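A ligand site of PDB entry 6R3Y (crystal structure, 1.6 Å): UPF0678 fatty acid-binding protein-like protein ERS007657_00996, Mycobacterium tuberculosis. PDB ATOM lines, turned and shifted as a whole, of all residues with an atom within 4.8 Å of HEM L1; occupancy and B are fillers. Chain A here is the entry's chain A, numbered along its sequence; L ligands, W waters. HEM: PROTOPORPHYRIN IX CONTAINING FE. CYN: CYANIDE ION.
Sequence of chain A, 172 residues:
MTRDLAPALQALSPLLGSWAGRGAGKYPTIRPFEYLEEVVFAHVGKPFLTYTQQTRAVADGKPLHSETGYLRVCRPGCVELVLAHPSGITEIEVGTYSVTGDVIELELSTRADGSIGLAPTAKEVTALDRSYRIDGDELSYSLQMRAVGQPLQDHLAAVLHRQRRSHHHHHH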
ATOM      1  N   TYR A  27     -14.608   9.901  27.043  1.00  0.00           N
ATOM      2  CA  TYR A  27     -13.339  10.502  27.472  1.00  0.00           C
ATOM      3  C   TYR A  27     -13.589  11.289  28.748  1.00  0.00           C
ATOM      4  O   TYR A  27     -14.723  11.705  28.969  1.00  0.00           O
ATOM      5  CB  TYR A  27     -12.732  11.388  26.363  1.00  0.00           C
ATOM      6  CG  TYR A  27     -11.219  11.344  26.317  1.00  0.00           C
ATOM      7  CD1 TYR A  27     -10.545  10.135  26.143  1.00  0.00           C
ATOM      8  CD2 TYR A  27     -10.461  12.475  26.560  1.00  0.00           C
ATOM      9  CE1 TYR A  27      -9.159  10.071  26.179  1.00  0.00           C
ATOM     10  CE2 TYR A  27      -9.072  12.433  26.565  1.00  0.00           C
ATOM     11  CZ  TYR A  27      -8.412  11.223  26.392  1.00  0.00           C
ATOM     12  OH  TYR A  27      -7.047  11.134  26.483  1.00  0.00           O
ATOM     13  N   THR A  29     -13.311  14.156  29.684  1.00  0.00           N
ATOM     14  CA  THR A  29     -13.632  15.594  29.506  1.00  0.00           C
ATOM     15  C   THR A  29     -14.986  15.754  28.813  1.00  0.00           C
ATOM     16  O   THR A  29     -15.408  16.911  28.638  1.00  0.00           O
ATOM     17  CB  THR A  29     -12.522  16.286  28.715  1.00  0.00           C
ATOM     18  OG1 THR A  29     -12.345  15.518  27.519  1.00  0.00           O
ATOM     19  CG2 THR A  29     -11.215  16.373  29.484  1.00  0.00           C
ATOM     20  N   ILE A  30     -15.651  14.656  28.455  1.00  0.00           N
ATOM     21  CA  ILE A  30     -16.869  14.665  27.593  1.00  0.00           C
ATOM     22  C   ILE A  30     -17.898  13.699  28.194  1.00  0.00           C
ATOM     23  O   ILE A  30     -17.528  12.896  29.063  1.00  0.00           O
ATOM     24  CB  ILE A  30     -16.550  14.309  26.123  1.00  0.00           C
ATOM     25  CG1 ILE A  30     -16.175  12.839  25.986  1.00  0.00           C
ATOM     26  CG2 ILE A  30     -15.456  15.240  25.577  1.00  0.00           C
ATOM     27  CD1 ILE A  30     -15.924  12.368  24.577  1.00  0.00           C
ATOM     28  N   PHE A  33     -20.997   8.548  24.333  1.00  0.00           N
ATOM     29  CA  PHE A  33     -21.756   8.613  23.078  1.00  0.00           C
ATOM     30  C   PHE A  33     -21.697   7.253  22.388  1.00  0.00           C
ATOM     31  O   PHE A  33     -20.832   6.392  22.747  1.00  0.00           O
ATOM     32  CB  PHE A  33     -21.197   9.704  22.138  1.00  0.00           C
ATOM     33  CG  PHE A  33     -19.740   9.524  21.798  1.00  0.00           C
ATOM     34  CD1 PHE A  33     -19.365   8.729  20.722  1.00  0.00           C
ATOM     35  CD2 PHE A  33     -18.742  10.040  22.619  1.00  0.00           C
ATOM     36  CE1 PHE A  33     -18.025   8.505  20.450  1.00  0.00           C
ATOM     37  CE2 PHE A  33     -17.410   9.812  22.341  1.00  0.00           C
ATOM     38  CZ  PHE A  33     -17.055   9.018  21.274  1.00  0.00           C
ATOM     39  N   TYR A  35     -22.271   5.622  18.099  1.00  0.00           N
ATOM     40  CA  TYR A  35     -22.186   6.042  16.693  1.00  0.00           C
ATOM     41  C   TYR A  35     -22.421   4.849  15.774  1.00  0.00           C
ATOM     42  O   TYR A  35     -22.109   3.688  16.152  1.00  0.00           O
ATOM     43  CB  TYR A  35     -20.842   6.730  16.451  1.00  0.00           C
ATOM     44  CG  TYR A  35     -19.615   5.885  16.724  1.00  0.00           C
ATOM     45  CD1 TYR A  35     -19.028   5.115  15.727  1.00  0.00           C
ATOM     46  CD2 TYR A  35     -19.001   5.903  17.963  1.00  0.00           C
ATOM     47  CE1 TYR A  35     -17.866   4.384  15.954  1.00  0.00           C
ATOM     48  CE2 TYR A  35     -17.820   5.200  18.201  1.00  0.00           C
ATOM     49  CZ  TYR A  35     -17.248   4.433  17.188  1.00  0.00           C
ATOM     50  OH  TYR A  35     -16.082   3.758  17.448  1.00  0.00           O
ATOM     51  N   GLU A  37     -21.016   3.523  11.935  1.00  0.00           N
ATOM     52  CA  GLU A  37     -19.736   3.644  11.220  1.00  0.00           C
ATOM     53  C   GLU A  37     -19.809   2.900   9.884  1.00  0.00           C
ATOM     54  O   GLU A  37     -20.278   1.780   9.864  1.00  0.00           O
ATOM     55  CB  GLU A  37     -18.602   3.108  12.078  1.00  0.00           C
ATOM     56  CG  GLU A  37     -17.267   3.184  11.369  1.00  0.00           C
ATOM     57  CD  GLU A  37     -16.097   2.923  12.290  1.00  0.00           C
ATOM     58  OE1 GLU A  37     -16.348   2.707  13.494  1.00  0.00           O
ATOM     59  OE2 GLU A  37     -14.953   2.875  11.781  1.00  0.00           O
ATOM     60  N   GLN A  53     -13.463   6.521   6.458  1.00  0.00           N
ATOM     61  CA  GLN A  53     -14.445   6.241   7.542  1.00  0.00           C
ATOM     62  C   GLN A  53     -15.418   7.413   7.602  1.00  0.00           C
ATOM     63  O   GLN A  53     -14.954   8.557   7.515  1.00  0.00           O
ATOM     64  CB  GLN A  53     -13.718   6.063   8.878  1.00  0.00           C
ATOM     65  CG  GLN A  53     -14.662   5.911  10.063  1.00  0.00           C
ATOM     66  CD  GLN A  53     -14.082   6.456  11.348  1.00  0.00           C
ATOM     67  OE1 GLN A  53     -13.730   5.713  12.241  1.00  0.00           O
ATOM     68  NE2 GLN A  53     -13.961   7.767  11.428  1.00  0.00           N
ATOM     69  N   THR A  55     -18.704   8.438  10.320  1.00  0.00           N
ATOM     70  CA  THR A  55     -19.556   8.049  11.468  1.00  0.00           C
ATOM     71  C   THR A  55     -20.705   9.037  11.590  1.00  0.00           C
ATOM     72  O   THR A  55     -20.531  10.206  11.146  1.00  0.00           O
ATOM     73  CB  THR A  55     -18.763   7.895  12.761  1.00  0.00           C
ATOM     74  OG1 THR A  55     -18.375   9.200  13.199  1.00  0.00           O
ATOM     75  CG2 THR A  55     -17.557   6.982  12.562  1.00  0.00           C
ATOM     76  N   LEU A  64     -20.784  12.755  12.665  1.00  0.00           N
ATOM     77  CA  LEU A  64     -19.867  12.994  13.783  1.00  0.00           C
ATOM     78  C   LEU A  64     -18.457  13.057  13.189  1.00  0.00           C
ATOM     79  O   LEU A  64     -18.217  13.945  12.363  1.00  0.00           O
ATOM     80  CB  LEU A  64     -20.081  11.902  14.835  1.00  0.00           C
ATOM     81  CG  LEU A  64     -21.466  11.913  15.476  1.00  0.00           C
ATOM     82  CD1 LEU A  64     -21.712  10.678  16.326  1.00  0.00           C
ATOM     83  CD2 LEU A  64     -21.659  13.171  16.317  1.00  0.00           C
ATOM     84  N   HIS A  65     -17.639  12.056  13.413  1.00  0.00           N
ATOM     85  CA  HIS A  65     -16.222  12.065  12.990  1.00  0.00           C
ATOM     86  C   HIS A  65     -16.139  11.430  11.605  1.00  0.00           C
ATOM     87  O   HIS A  65     -17.012  10.622  11.233  1.00  0.00           O
ATOM     88  CB  HIS A  65     -15.362  11.359  14.039  1.00  0.00           C
ATOM     89  CG  HIS A  65     -13.911  11.332  13.710  1.00  0.00           C
ATOM     90  ND1 HIS A  65     -13.302  10.205  13.139  1.00  0.00           N
ATOM     91  CD2 HIS A  65     -12.931  12.234  13.951  1.00  0.00           C
ATOM     92  CE1 HIS A  65     -12.012  10.450  12.996  1.00  0.00           C
ATOM     93  NE2 HIS A  65     -11.761  11.709  13.444  1.00  0.00           N
ATOM     94  N   GLU A  67     -12.566  10.147   8.870  1.00  0.00           N
ATOM     95  CA  GLU A  67     -11.110  10.119   8.685  1.00  0.00           C
ATOM     96  C   GLU A  67     -10.800   9.467   7.348  1.00  0.00           C
ATOM     97  O   GLU A  67     -11.656   8.774   6.811  1.00  0.00           O
ATOM     98  CB  GLU A  67     -10.397   9.428   9.857  1.00  0.00           C
ATOM     99  CG  GLU A  67     -10.897   8.034  10.152  1.00  0.00           C
ATOM    100  CD  GLU A  67     -10.260   7.343  11.351  1.00  0.00           C
ATOM    101  OE1 GLU A  67      -9.929   8.043  12.327  1.00  0.00           O
ATOM    102  OE2 GLU A  67     -10.181   6.095  11.342  1.00  0.00           O
ATOM    103  N   HIS A  85      -7.868  14.155   9.676  1.00  0.00           N
ATOM    104  CA  HIS A  85      -9.105  14.316  10.472  1.00  0.00           C
ATOM    105  C   HIS A  85      -9.705  15.690  10.219  1.00  0.00           C
ATOM    106  O   HIS A  85      -8.998  16.691  10.210  1.00  0.00           O
ATOM    107  CB  HIS A  85      -8.821  14.133  11.953  1.00  0.00           C
ATOM    108  CG  HIS A  85      -8.261  12.789  12.273  1.00  0.00           C
ATOM    109  ND1 HIS A  85      -9.061  11.730  12.625  1.00  0.00           N
ATOM    110  CD2 HIS A  85      -7.000  12.322  12.307  1.00  0.00           C
ATOM    111  CE1 HIS A  85      -8.329  10.665  12.856  1.00  0.00           C
ATOM    112  NE2 HIS A  85      -7.061  10.986  12.633  1.00  0.00           N
ATOM    113  N   ILE A  89      -6.481  17.685  12.619  1.00  0.00           N
ATOM    114  CA  ILE A  89      -5.427  16.826  13.179  1.00  0.00           C
ATOM    115  C   ILE A  89      -4.986  15.820  12.118  1.00  0.00           C
ATOM    116  O   ILE A  89      -5.843  15.342  11.320  1.00  0.00           O
ATOM    117  CB  ILE A  89      -5.930  16.119  14.450  1.00  0.00           C
ATOM    118  CG1 ILE A  89      -6.329  17.144  15.517  1.00  0.00           C
ATOM    119  CG2 ILE A  89      -4.912  15.138  14.951  1.00  0.00           C
ATOM    120  CD1 ILE A  89      -6.976  16.536  16.728  1.00  0.00           C
ATOM    121  N   LYS A 123      -7.868  20.796  19.048  1.00  0.00           N
ATOM    122  CA  LYS A 123      -7.673  20.262  20.423  1.00  0.00           C
ATOM    123  C   LYS A 123      -6.338  19.538  20.518  1.00  0.00           C
ATOM    124  O   LYS A 123      -5.858  19.019  19.485  1.00  0.00           O
ATOM    125  CB  LYS A 123      -8.810  19.302  20.786  1.00  0.00           C
ATOM    126  CG  LYS A 123     -10.196  19.937  20.817  1.00  0.00           C
ATOM    127  CD  LYS A 123     -10.444  20.746  22.062  1.00  0.00           C
ATOM    128  CE  LYS A 123     -11.773  21.476  22.040  1.00  0.00           C
ATOM    129  NZ  LYS A 123     -12.910  20.542  21.857  1.00  0.00           N
ATOM    130  N   VAL A 125      -4.244  16.739  21.006  1.00  0.00           N
ATOM    131  CA  VAL A 125      -4.065  15.262  20.980  1.00  0.00           C
ATOM    132  C   VAL A 125      -2.570  14.981  20.879  1.00  0.00           C
ATOM    133  O   VAL A 125      -1.930  15.574  19.983  1.00  0.00           O
ATOM    134  CB  VAL A 125      -4.846  14.620  19.823  1.00  0.00           C
ATOM    135  CG1 VAL A 125      -4.589  13.120  19.764  1.00  0.00           C
ATOM    136  CG2 VAL A 125      -6.331  14.886  19.937  1.00  0.00           C
ATOM    137  N   LEU A 128      -2.193   8.387  19.899  1.00  0.00           N
ATOM    138  CA  LEU A 128      -3.311   7.519  19.508  1.00  0.00           C
ATOM    139  C   LEU A 128      -2.793   6.109  19.281  1.00  0.00           C
ATOM    140  O   LEU A 128      -1.732   5.960  18.610  1.00  0.00           O
ATOM    141  CB  LEU A 128      -3.959   8.045  18.243  1.00  0.00           C
ATOM    142  CG  LEU A 128      -4.653   9.403  18.363  1.00  0.00           C
ATOM    143  CD1 LEU A 128      -4.838  10.045  16.986  1.00  0.00           C
ATOM    144  CD2 LEU A 128      -5.983   9.289  19.085  1.00  0.00           C
ATOM    145  N   ARG A 130      -4.215   2.174  18.091  1.00  0.00           N
ATOM    146  CA  ARG A 130      -5.315   1.403  17.460  1.00  0.00           C
ATOM    147  C   ARG A 130      -5.000  -0.083  17.506  1.00  0.00           C
ATOM    148  O   ARG A 130      -3.874  -0.460  17.158  1.00  0.00           O
ATOM    149  CB  ARG A 130      -5.523   1.884  16.031  1.00  0.00           C
ATOM    150  CG  ARG A 130      -6.124   3.264  15.941  1.00  0.00           C
ATOM    151  CD  ARG A 130      -6.159   3.709  14.501  1.00  0.00           C
ATOM    152  NE  ARG A 130      -6.473   5.124  14.376  1.00  0.00           N
ATOM    153  CZ  ARG A 130      -7.562   5.596  13.796  1.00  0.00           C
ATOM    154  NH1 ARG A 130      -8.466   4.767  13.289  1.00  0.00           N
ATOM    155  NH2 ARG A 130      -7.709   6.904  13.671  1.00  0.00           N
ATOM    156  N   TYR A 141     -12.412  -3.023  16.632  1.00  0.00           N
ATOM    157  CA  TYR A 141     -11.240  -2.209  17.001  1.00  0.00           C
ATOM    158  C   TYR A 141     -11.513  -1.516  18.321  1.00  0.00           C
ATOM    159  O   TYR A 141     -12.686  -1.311  18.683  1.00  0.00           O
ATOM    160  CB  TYR A 141     -10.901  -1.207  15.894  1.00  0.00           C
ATOM    161  CG  TYR A 141     -11.883  -0.074  15.734  1.00  0.00           C
ATOM    162  CD1 TYR A 141     -11.846   1.031  16.575  1.00  0.00           C
ATOM    163  CD2 TYR A 141     -12.828  -0.078  14.712  1.00  0.00           C
ATOM    164  CE1 TYR A 141     -12.773   2.061  16.436  1.00  0.00           C
ATOM    165  CE2 TYR A 141     -13.699   0.983  14.520  1.00  0.00           C
ATOM    166  CZ  TYR A 141     -13.677   2.057  15.396  1.00  0.00           C
ATOM    167  OH  TYR A 141     -14.589   3.059  15.236  1.00  0.00           O
ATOM    168  N   LEU A 143      -9.638   2.138  20.136  1.00  0.00           N
ATOM    169  CA  LEU A 143      -8.724   3.274  19.953  1.00  0.00           C
ATOM    170  C   LEU A 143      -8.517   3.906  21.316  1.00  0.00           C
ATOM    171  O   LEU A 143      -9.534   4.193  21.995  1.00  0.00           O
ATOM    172  CB  LEU A 143      -9.316   4.255  18.946  1.00  0.00           C
ATOM    173  CG  LEU A 143      -8.470   5.510  18.701  1.00  0.00           C
ATOM    174  CD1 LEU A 143      -8.674   6.012  17.271  1.00  0.00           C
ATOM    175  CD2 LEU A 143      -8.801   6.585  19.708  1.00  0.00           C
ATOM    176  N   MET A 145      -6.529   7.090  23.391  1.00  0.00           N
ATOM    177  CA  MET A 145      -6.099   8.464  23.092  1.00  0.00           C
ATOM    178  C   MET A 145      -5.435   9.053  24.319  1.00  0.00           C
ATOM    179  O   MET A 145      -5.984   8.902  25.453  1.00  0.00           O
ATOM    180  CB  MET A 145      -7.297   9.324  22.675  1.00  0.00           C
ATOM    181  CG  MET A 145      -6.958  10.784  22.409  1.00  0.00           C
ATOM    182  SD  MET A 145      -8.315  11.617  21.534  1.00  0.00           S
ATOM    183  CE  MET A 145      -9.608  11.651  22.766  1.00  0.00           C
ATOM    184  N   ALA A 147      -4.743  12.920  25.322  1.00  0.00           N
ATOM    185  CA  ALA A 147      -5.222  14.240  24.849  1.00  0.00           C
ATOM    186  C   ALA A 147      -5.752  15.091  26.017  1.00  0.00           C
ATOM    187  O   ALA A 147      -6.163  14.514  27.023  1.00  0.00           O
ATOM    188  CB  ALA A 147      -6.299  14.046  23.821  1.00  0.00           C
ATOM    189  N   VAL A 148      -5.720  16.407  25.820  1.00  0.00           N
ATOM    190  CA  VAL A 148      -6.402  17.422  26.671  1.00  0.00           C
ATOM    191  C   VAL A 148      -6.206  17.043  28.147  1.00  0.00           C
ATOM    192  O   VAL A 148      -7.172  17.134  28.948  1.00  0.00           O
ATOM    193  CB  VAL A 148      -7.880  17.585  26.264  1.00  0.00           C
ATOM    194  CG1 VAL A 148      -8.012  18.201  24.886  1.00  0.00           C
ATOM    195  CG2 VAL A 148      -8.688  16.292  26.333  1.00  0.00           C
ATOM    196  N   HIS A 155     -10.926   5.828  23.973  1.00  0.00           N
ATOM    197  CA  HIS A 155     -11.877   6.825  23.432  1.00  0.00           C
ATOM    198  C   HIS A 155     -12.978   6.091  22.667  1.00  0.00           C
ATOM    199  O   HIS A 155     -14.099   6.610  22.667  1.00  0.00           O
ATOM    200  CB  HIS A 155     -11.143   7.890  22.590  1.00  0.00           C
ATOM    201  CG  HIS A 155     -12.027   8.939  21.989  1.00  0.00           C
ATOM    202  ND1 HIS A 155     -13.015   9.579  22.746  1.00  0.00           N
ATOM    203  CD2 HIS A 155     -11.995   9.566  20.787  1.00  0.00           C
ATOM    204  CE1 HIS A 155     -13.559  10.537  22.009  1.00  0.00           C
ATOM    205  NE2 HIS A 155     -12.994  10.506  20.783  1.00  0.00           N
ATOM    206  N   LEU A 156     -12.647   5.034  21.917  1.00  0.00           N
ATOM    207  CA  LEU A 156     -13.588   4.395  20.972  1.00  0.00           C
ATOM    208  C   LEU A 156     -13.454   2.886  21.051  1.00  0.00           C
ATOM    209  O   LEU A 156     -12.342   2.400  21.144  1.00  0.00           O
ATOM    210  CB  LEU A 156     -13.300   4.818  19.531  1.00  0.00           C
ATOM    211  CG  LEU A 156     -13.221   6.318  19.264  1.00  0.00           C
ATOM    212  CD1 LEU A 156     -12.668   6.545  17.867  1.00  0.00           C
ATOM    213  CD2 LEU A 156     -14.570   6.972  19.422  1.00  0.00           C
HETATM  214  CHA HEM L   1     -14.507  14.300  21.610  1.00  0.00           C
HETATM  215  CHB HEM L   1     -16.816  11.176  18.699  1.00  0.00           C
HETATM  216  CHC HEM L   1     -12.571   9.749  16.798  1.00  0.00           C
HETATM  217  CHD HEM L   1     -10.325  13.189  19.421  1.00  0.00           C
HETATM  218  C1A HEM L   1     -15.465  13.548  20.980  1.00  0.00           C
HETATM  219  C2A HEM L   1     -16.865  13.752  21.187  1.00  0.00           C
HETATM  220  C3A HEM L   1     -17.512  12.899  20.344  1.00  0.00           C
HETATM  221  C4A HEM L   1     -16.529  12.137  19.641  1.00  0.00           C
HETATM  222  CMA HEM L   1     -19.014  12.765  20.222  1.00  0.00           C
HETATM  223  CAA HEM L   1     -17.536  14.751  22.134  1.00  0.00           C
HETATM  224  CBA HEM L   1     -18.200  15.886  21.368  1.00  0.00           C
HETATM  225  CGA HEM L   1     -17.140  16.710  20.720  1.00  0.00           C
HETATM  226  O1A HEM L   1     -17.147  16.885  19.470  1.00  0.00           O
HETATM  227  O2A HEM L   1     -16.187  17.145  21.423  1.00  0.00           O
HETATM  228  C1B HEM L   1     -15.846  10.503  17.947  1.00  0.00           C
HETATM  229  C2B HEM L   1     -16.157   9.483  16.998  1.00  0.00           C
HETATM  230  C3B HEM L   1     -14.951   9.053  16.447  1.00  0.00           C
HETATM  231  C4B HEM L   1     -13.923   9.860  17.114  1.00  0.00           C
HETATM  232  CMB HEM L   1     -17.555   9.038  16.662  1.00  0.00           C
HETATM  233  CAB HEM L   1     -14.650   7.998  15.449  1.00  0.00           C
HETATM  234  CBB HEM L   1     -15.442   6.928  15.299  1.00  0.00           C
HETATM  235  C1C HEM L   1     -11.586  10.633  17.310  1.00  0.00           C
HETATM  236  C2C HEM L   1     -10.251  10.670  16.873  1.00  0.00           C
HETATM  237  C3C HEM L   1      -9.605  11.648  17.616  1.00  0.00           C
HETATM  238  C4C HEM L   1     -10.585  12.191  18.514  1.00  0.00           C
HETATM  239  CMC HEM L   1      -9.667   9.761  15.851  1.00  0.00           C
HETATM  240  CAC HEM L   1      -8.252  12.186  17.460  1.00  0.00           C
HETATM  241  CBC HEM L   1      -7.670  12.308  16.266  1.00  0.00           C
HETATM  242  C1D HEM L   1     -11.292  13.750  20.244  1.00  0.00           C
HETATM  243  C2D HEM L   1     -10.980  14.834  21.192  1.00  0.00           C
HETATM  244  C3D HEM L   1     -12.141  15.141  21.802  1.00  0.00           C
HETATM  245  C4D HEM L   1     -13.172  14.238  21.225  1.00  0.00           C
HETATM  246  CMD HEM L   1      -9.638  15.530  21.416  1.00  0.00           C
HETATM  247  CAD HEM L   1     -12.416  16.337  22.678  1.00  0.00           C
HETATM  248  CBD HEM L   1     -12.168  16.114  24.123  1.00  0.00           C
HETATM  249  CGD HEM L   1     -12.359  17.463  24.832  1.00  0.00           C
HETATM  250  O1D HEM L   1     -12.848  18.506  24.250  1.00  0.00           O
HETATM  251  O2D HEM L   1     -11.982  17.554  25.972  1.00  0.00           O
HETATM  252  NA  HEM L   1     -15.289  12.525  20.052  1.00  0.00           N
HETATM  253  NB  HEM L   1     -14.512  10.686  18.000  1.00  0.00           N
HETATM  254  NC  HEM L   1     -11.764  11.563  18.273  1.00  0.00           N
HETATM  255  ND  HEM L   1     -12.623  13.419  20.315  1.00  0.00           N
HETATM  256 FE   HEM L   1     -13.511  12.021  19.272  1.00  0.00          FE
HETATM  257  C   CYN L   2     -13.837  13.507  17.641  1.00  0.00           C
HETATM  258  N   CYN L   2     -14.377  14.682  17.352  1.00  0.00           N
HETATM  259  O   HOH W   1     -11.037  19.518  27.399  1.00  0.00           O
HETATM  260  O   HOH W   2     -11.710   7.341  14.243  1.00  0.00           O
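A ring nitrogen (NE2) of His 155 binds an iron atom (FE) of HEM L1, 2.2 Å away. An oxygen (O2D) of HEM L1 is in hydrogen-bond range of the side-chain hydroxyl (OG1) of Thr 29 (2.6 Å). The side-chain amino group (NZ) of Lys 123 is in salt-bridge range of an oxygen (O1D) of HEM L1 (3.1 Å).
The backbone NH (N) of His 155 lies within hydrogen-bond range of the backbone carbonyl oxygen (O) of Leu 143 (2.9 Å). The backbone carbonyl oxygen (O) of Met 145 is in hydrogen-bond range of the side-chain hydroxyl (OH) of Tyr 27. A ring nitrogen (NE2) of His 65 is in hydrogen-bond range of a ring nitrogen (ND1) of His 85 (2.8 Å). The backbone carbonyl oxygen of Leu 156 lies within hydrogen-bond range of the backbone NH of Leu 143 (2.9 Å). The backbone carbonyl oxygen (O) of Thr 55 is in hydrogen-bond range of the backbone NH (N) of Leu 64 (3.0 Å). The backbone carbonyl oxygen of Glu 67 is in hydrogen-bond range of the backbone NH of Gln 53, at 2.9 Å. The side-chain carboxylate of Glu 67 is in salt-bridge range of the guanidinium group of Arg 130. The side-chain carboxylate (OE1) of Glu 37 lies within hydrogen-bond range of the side-chain hydroxyl (OH) of Tyr 141, at 2.5 Å.
Residues that only touch HEM L1: Ile 30 (3.7 Å), Phe 33 (3.4 Å), Tyr 35 (3.6 Å), Gln 53 (3.7 Å), Thr 55 (3.5 Å), His 65 (3.4 Å), Glu 67 (3.9 Å), His 85 (3.4 Å), Val 125 (3.7 Å), Leu 128 (3.7 Å), Tyr 141 (3.96 Å), Met 145 (3.3 Å), Val 148 (3.5 Å) and Leu 156 (3.4 Å). Hydrophobic or aromatic side chains within 4 Å of HEM L1: Ile 30, Phe 33, Tyr 35, His 65, His 85, Val 125, Leu 128, Met 145, Val 148, His 155 and Leu 156. Of the 24 residues printed, 17 come within 4 Å of HEM L1. The nearest printed residue that does not touch HEM L1 is Arg 130 (4.1 Å).
Water W2 lies within hydrogen-bond range of OE1 of Glu 67 (2.7 Å), OE1 of Gln 53 (3.3 Å) and ND1 of His 65 (3.5 Å).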
